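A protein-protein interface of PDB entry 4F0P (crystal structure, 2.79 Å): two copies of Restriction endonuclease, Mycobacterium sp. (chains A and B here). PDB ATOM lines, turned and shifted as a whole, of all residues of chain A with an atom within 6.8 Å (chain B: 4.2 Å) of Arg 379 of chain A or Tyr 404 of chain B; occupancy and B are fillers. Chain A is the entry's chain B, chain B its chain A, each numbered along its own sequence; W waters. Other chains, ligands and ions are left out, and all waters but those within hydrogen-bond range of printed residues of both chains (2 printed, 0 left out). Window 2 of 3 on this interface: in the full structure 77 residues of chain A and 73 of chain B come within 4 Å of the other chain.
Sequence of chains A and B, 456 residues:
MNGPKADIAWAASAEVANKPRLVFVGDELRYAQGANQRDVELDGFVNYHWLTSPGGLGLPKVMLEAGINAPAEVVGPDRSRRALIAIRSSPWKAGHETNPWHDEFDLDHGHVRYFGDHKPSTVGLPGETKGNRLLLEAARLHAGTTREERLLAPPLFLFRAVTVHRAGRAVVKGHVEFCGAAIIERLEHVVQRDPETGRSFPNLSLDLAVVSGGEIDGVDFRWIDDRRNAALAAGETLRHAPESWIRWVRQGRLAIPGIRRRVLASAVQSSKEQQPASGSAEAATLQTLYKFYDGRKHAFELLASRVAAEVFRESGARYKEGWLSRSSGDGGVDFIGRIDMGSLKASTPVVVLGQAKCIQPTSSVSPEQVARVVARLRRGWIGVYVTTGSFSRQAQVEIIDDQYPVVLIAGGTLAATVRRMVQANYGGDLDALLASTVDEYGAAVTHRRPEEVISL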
ATOM      1  N   THR A 348     -31.169 -33.969 -20.622  1.00  0.00           N
ATOM      2  CA  THR A 348     -29.941 -33.638 -21.333  1.00  0.00           C
ATOM      3  C   THR A 348     -28.868 -33.172 -20.346  1.00  0.00           C
ATOM      4  O   THR A 348     -29.171 -32.472 -19.378  1.00  0.00           O
ATOM      5  CB  THR A 348     -30.185 -32.576 -22.440  1.00  0.00           C
ATOM      6  OG1 THR A 348     -29.003 -32.418 -23.234  1.00  0.00           O
ATOM      7  CG2 THR A 348     -30.581 -31.231 -21.841  1.00  0.00           C
ATOM      8  N   PRO A 349     -27.612 -33.588 -20.572  1.00  0.00           N
ATOM      9  CA  PRO A 349     -26.507 -33.212 -19.683  1.00  0.00           C
ATOM     10  C   PRO A 349     -26.083 -31.759 -19.863  1.00  0.00           C
ATOM     11  O   PRO A 349     -25.964 -31.280 -20.992  1.00  0.00           O
ATOM     12  CB  PRO A 349     -25.377 -34.145 -20.120  1.00  0.00           C
ATOM     13  CG  PRO A 349     -25.675 -34.445 -21.546  1.00  0.00           C
ATOM     14  CD  PRO A 349     -27.173 -34.509 -21.635  1.00  0.00           C
ATOM     15  N   LEU A 377     -17.187 -20.886 -21.331  1.00  0.00           N
ATOM     16  CA  LEU A 377     -18.491 -21.535 -21.457  1.00  0.00           C
ATOM     17  C   LEU A 377     -18.932 -21.772 -22.900  1.00  0.00           C
ATOM     18  O   LEU A 377     -19.040 -20.836 -23.694  1.00  0.00           O
ATOM     19  CB  LEU A 377     -19.562 -20.727 -20.720  1.00  0.00           C
ATOM     20  CG  LEU A 377     -19.410 -20.598 -19.204  1.00  0.00           C
ATOM     21  CD1 LEU A 377     -20.488 -19.682 -18.642  1.00  0.00           C
ATOM     22  CD2 LEU A 377     -19.454 -21.966 -18.532  1.00  0.00           C
ATOM     23  N   ARG A 378     -19.187 -23.036 -23.228  1.00  0.00           N
ATOM     24  CA  ARG A 378     -19.806 -23.393 -24.496  1.00  0.00           C
ATOM     25  C   ARG A 378     -21.315 -23.381 -24.303  1.00  0.00           C
ATOM     26  O   ARG A 378     -21.806 -22.988 -23.248  1.00  0.00           O
ATOM     27  CB  ARG A 378     -19.347 -24.779 -24.951  1.00  0.00           C
ATOM     28  CG  ARG A 378     -17.850 -24.897 -25.182  1.00  0.00           C
ATOM     29  CD  ARG A 378     -17.493 -26.273 -25.726  1.00  0.00           C
ATOM     30  NE  ARG A 378     -16.069 -26.400 -26.024  1.00  0.00           N
ATOM     31  CZ  ARG A 378     -15.509 -27.490 -26.539  1.00  0.00           C
ATOM     32  NH1 ARG A 378     -16.253 -28.552 -26.817  1.00  0.00           N
ATOM     33  NH2 ARG A 378     -14.204 -27.518 -26.779  1.00  0.00           N
ATOM     34  N   ARG A 379     -22.057 -23.810 -25.316  1.00  0.00           N
ATOM     35  CA  ARG A 379     -23.508 -23.863 -25.186  1.00  0.00           C
ATOM     36  C   ARG A 379     -23.925 -25.175 -24.538  1.00  0.00           C
ATOM     37  O   ARG A 379     -23.321 -26.220 -24.778  1.00  0.00           O
ATOM     38  CB  ARG A 379     -24.196 -23.683 -26.536  1.00  0.00           C
ATOM     39  CG  ARG A 379     -23.991 -24.828 -27.495  1.00  0.00           C
ATOM     40  CD  ARG A 379     -24.733 -24.576 -28.782  1.00  0.00           C
ATOM     41  NE  ARG A 379     -24.560 -25.672 -29.722  1.00  0.00           N
ATOM     42  CZ  ARG A 379     -24.949 -25.628 -30.990  1.00  0.00           C
ATOM     43  NH1 ARG A 379     -25.530 -24.535 -31.470  1.00  0.00           N
ATOM     44  NH2 ARG A 379     -24.754 -26.674 -31.776  1.00  0.00           N
ATOM     45  N   GLY A 380     -24.958 -25.113 -23.709  1.00  0.00           N
ATOM     46  CA  GLY A 380     -25.348 -26.257 -22.910  1.00  0.00           C
ATOM     47  C   GLY A 380     -24.483 -26.347 -21.669  1.00  0.00           C
ATOM     48  O   GLY A 380     -24.561 -27.311 -20.912  1.00  0.00           O
ATOM     49  N   TRP A 381     -23.646 -25.334 -21.467  1.00  0.00           N
ATOM     50  CA  TRP A 381     -22.810 -25.251 -20.277  1.00  0.00           C
ATOM     51  C   TRP A 381     -23.259 -24.083 -19.416  1.00  0.00           C
ATOM     52  O   TRP A 381     -23.723 -23.065 -19.933  1.00  0.00           O
ATOM     53  CB  TRP A 381     -21.338 -25.045 -20.643  1.00  0.00           C
ATOM     54  CG  TRP A 381     -20.704 -26.167 -21.403  1.00  0.00           C
ATOM     55  CD1 TRP A 381     -21.335 -27.133 -22.132  1.00  0.00           C
ATOM     56  CD2 TRP A 381     -19.303 -26.439 -21.506  1.00  0.00           C
ATOM     57  NE1 TRP A 381     -20.412 -27.988 -22.686  1.00  0.00           N
ATOM     58  CE2 TRP A 381     -19.156 -27.584 -22.316  1.00  0.00           C
ATOM     59  CE3 TRP A 381     -18.156 -25.825 -20.992  1.00  0.00           C
ATOM     60  CZ2 TRP A 381     -17.909 -28.127 -22.623  1.00  0.00           C
ATOM     61  CZ3 TRP A 381     -16.918 -26.366 -21.299  1.00  0.00           C
ATOM     62  CH2 TRP A 381     -16.805 -27.506 -22.108  1.00  0.00           C
ATOM     63  N   ILE A 382     -23.120 -24.232 -18.104  1.00  0.00           N
ATOM     64  CA  ILE A 382     -23.358 -23.126 -17.186  1.00  0.00           C
ATOM     65  C   ILE A 382     -22.162 -22.955 -16.256  1.00  0.00           C
ATOM     66  O   ILE A 382     -21.426 -23.907 -15.993  1.00  0.00           O
ATOM     67  CB  ILE A 382     -24.643 -23.322 -16.354  1.00  0.00           C
ATOM     68  CG1 ILE A 382     -24.575 -24.626 -15.558  1.00  0.00           C
ATOM     69  CG2 ILE A 382     -25.871 -23.307 -17.253  1.00  0.00           C
ATOM     70  CD1 ILE A 382     -25.812 -24.894 -14.728  1.00  0.00           C
ATOM     71  N   VAL B 374     -31.690 -26.461 -32.650  1.00  0.00           N
ATOM     72  CA  VAL B 374     -30.383 -26.318 -32.011  1.00  0.00           C
ATOM     73  C   VAL B 374     -29.639 -25.059 -32.473  1.00  0.00           C
ATOM     74  O   VAL B 374     -28.976 -24.389 -31.677  1.00  0.00           O
ATOM     75  CB  VAL B 374     -29.504 -27.569 -32.239  1.00  0.00           C
ATOM     76  CG1 VAL B 374     -28.130 -27.385 -31.617  1.00  0.00           C
ATOM     77  CG2 VAL B 374     -30.183 -28.803 -31.667  1.00  0.00           C
ATOM     78  N   GLU B 398     -26.140 -37.407 -33.456  1.00  0.00           N
ATOM     79  CA  GLU B 398     -25.577 -36.068 -33.610  1.00  0.00           C
ATOM     80  C   GLU B 398     -25.766 -35.215 -32.358  1.00  0.00           C
ATOM     81  O   GLU B 398     -24.911 -34.392 -32.028  1.00  0.00           O
ATOM     82  CB  GLU B 398     -26.170 -35.366 -34.833  1.00  0.00           C
ATOM     83  CG  GLU B 398     -25.833 -36.053 -36.145  1.00  0.00           C
ATOM     84  CD  GLU B 398     -26.387 -35.324 -37.350  1.00  0.00           C
ATOM     85  OE1 GLU B 398     -26.412 -35.926 -38.444  1.00  0.00           O
ATOM     86  OE2 GLU B 398     -26.793 -34.151 -37.205  1.00  0.00           O
ATOM     87  N   ILE B 399     -26.886 -35.407 -31.669  1.00  0.00           N
ATOM     88  CA  ILE B 399     -27.124 -34.722 -30.401  1.00  0.00           C
ATOM     89  C   ILE B 399     -26.078 -35.138 -29.367  1.00  0.00           C
ATOM     90  O   ILE B 399     -25.558 -34.305 -28.625  1.00  0.00           O
ATOM     91  CB  ILE B 399     -28.543 -35.003 -29.864  1.00  0.00           C
ATOM     92  CG1 ILE B 399     -29.583 -34.327 -30.758  1.00  0.00           C
ATOM     93  CG2 ILE B 399     -28.689 -34.514 -28.427  1.00  0.00           C
ATOM     94  CD1 ILE B 399     -30.996 -34.774 -30.486  1.00  0.00           C
ATOM     95  N   ASP B 402     -22.077 -34.017 -31.076  1.00  0.00           N
ATOM     96  CA  ASP B 402     -21.810 -32.586 -31.042  1.00  0.00           C
ATOM     97  C   ASP B 402     -22.339 -31.937 -29.767  1.00  0.00           C
ATOM     98  O   ASP B 402     -22.268 -30.718 -29.610  1.00  0.00           O
ATOM     99  CB  ASP B 402     -22.401 -31.908 -32.278  1.00  0.00           C
ATOM    100  CG  ASP B 402     -21.876 -32.502 -33.570  1.00  0.00           C
ATOM    101  OD1 ASP B 402     -22.538 -33.402 -34.135  1.00  0.00           O
ATOM    102  OD2 ASP B 402     -20.793 -32.073 -34.017  1.00  0.00           O
ATOM    103  N   GLN B 403     -22.868 -32.763 -28.867  1.00  0.00           N
ATOM    104  CA  GLN B 403     -23.313 -32.319 -27.550  1.00  0.00           C
ATOM    105  C   GLN B 403     -24.362 -31.216 -27.634  1.00  0.00           C
ATOM    106  O   GLN B 403     -24.134 -30.094 -27.184  1.00  0.00           O
ATOM    107  CB  GLN B 403     -22.121 -31.856 -26.710  1.00  0.00           C
ATOM    108  CG  GLN B 403     -20.997 -32.874 -26.626  1.00  0.00           C
ATOM    109  CD  GLN B 403     -19.803 -32.357 -25.852  1.00  0.00           C
ATOM    110  OE1 GLN B 403     -19.953 -31.637 -24.864  1.00  0.00           O
ATOM    111  NE2 GLN B 403     -18.606 -32.715 -26.302  1.00  0.00           N
ATOM    112  N   TYR B 404     -25.509 -31.543 -28.219  1.00  0.00           N
ATOM    113  CA  TYR B 404     -26.604 -30.588 -28.334  1.00  0.00           C
ATOM    114  C   TYR B 404     -27.461 -30.589 -27.071  1.00  0.00           C
ATOM    115  O   TYR B 404     -28.001 -31.628 -26.685  1.00  0.00           O
ATOM    116  CB  TYR B 404     -27.476 -30.906 -29.551  1.00  0.00           C
ATOM    117  CG  TYR B 404     -26.779 -30.744 -30.886  1.00  0.00           C
ATOM    118  CD1 TYR B 404     -25.683 -29.902 -31.026  1.00  0.00           C
ATOM    119  CD2 TYR B 404     -27.223 -31.432 -32.010  1.00  0.00           C
ATOM    120  CE1 TYR B 404     -25.050 -29.750 -32.249  1.00  0.00           C
ATOM    121  CE2 TYR B 404     -26.594 -31.287 -33.234  1.00  0.00           C
ATOM    122  CZ  TYR B 404     -25.507 -30.446 -33.348  1.00  0.00           C
ATOM    123  OH  TYR B 404     -24.880 -30.300 -34.565  1.00  0.00           O
ATOM    124  N   PRO B 405     -27.581 -29.424 -26.418  1.00  0.00           N
ATOM    125  CA  PRO B 405     -28.431 -29.275 -25.231  1.00  0.00           C
ATOM    126  C   PRO B 405     -29.913 -29.274 -25.596  1.00  0.00           C
ATOM    127  O   PRO B 405     -30.564 -28.229 -25.554  1.00  0.00           O
ATOM    128  CB  PRO B 405     -28.022 -27.909 -24.678  1.00  0.00           C
ATOM    129  CG  PRO B 405     -27.529 -27.158 -25.866  1.00  0.00           C
ATOM    130  CD  PRO B 405     -26.866 -28.178 -26.748  1.00  0.00           C
ATOM    131  N   VAL B 406     -30.438 -30.441 -25.955  1.00  0.00           N
ATOM    132  CA  VAL B 406     -31.838 -30.557 -26.339  1.00  0.00           C
ATOM    133  C   VAL B 406     -32.501 -31.766 -25.681  1.00  0.00           C
ATOM    134  O   VAL B 406     -31.971 -32.880 -25.711  1.00  0.00           O
ATOM    135  CB  VAL B 406     -32.003 -30.610 -27.880  1.00  0.00           C
ATOM    136  CG1 VAL B 406     -31.105 -31.680 -28.486  1.00  0.00           C
ATOM    137  CG2 VAL B 406     -33.459 -30.837 -28.261  1.00  0.00           C
HETATM  138  O   HOH W   1     -30.184 -34.946 -25.192  1.00  0.00           O
HETATM  139  O   HOH W   2     -26.457 -31.367 -23.697  1.00  0.00           O
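OG1 of Thr 348 of chain A touches O of Tyr 404 of chain B, 3.7 Å away. OG1 of Thr 348 of chain A touches CA of Pro 405 of chain B, at 3.8 Å. OG1 of Thr 348 of chain A touches N of Val 406 of chain B, 3.7 Å away. CE1 of Tyr 404 of chain B touches NH2 of Arg 379 of chain A, at 3.1 Å. Gly 380 of chain A touches Pro 405 of chain B.
Arg 379 of chain A touches two residues of chain B. Tyr 404 of chain B touches two residues of chain A. Printed residues of chain B within 4 Å of Thr 348 of chain A: Tyr 404 (3.7 Å), Pro 405 (3.8 Å) and Val 406 (3.7 Å). Of the printed residues of chain A, Val 406 of chain B touches Thr 348. Printed residues of chain B within 4 Å of Gly 380 of chain A: Pro 405 (3.6 Å). Of the printed residues of chain A, Val 374 of chain B touches Arg 379 (3.5 Å). The nearest residue of chain A that does not touch Tyr 404 of chain B is Pro 349 of chain A (5.9 Å).
No position is printed for both chains. Of the 6 pairs that touch across the chains among the printed residues, none has its exchanged pair printed and touching as well.
N of Tyr 404 of chain B is in hydrogen-bond range of O of Ile 399 of chain B (2.8 Å).
Water W2 lies within hydrogen-bond range of O of Pro 349 of chain A, OG1 of Thr 348 of chain A and O of Tyr 404 of chain B. Water W1 bridges the backbone carbonyl oxygen (O) of Val 406 of chain B (2.8 Å) and the side-chain hydroxyl (OG1) of Thr 348 of chain A (3.4 Å).
Hydrophobic or aromatic side chains of chain B that line the printed part of chain A: Val 374, Tyr 404 and Pro 405. Printed residues of chain A that touch a printed residue of chain B: Thr 348, Arg 379 and Gly 380. Among the printed residues, 6 pairs touch across the chains.
The backbone carbonyl oxygen (O) of Val 374 of chain B is in hydrogen-bond range of the guanidinium group (NH1) of Arg 379 of chain A, 3.5 Å away.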
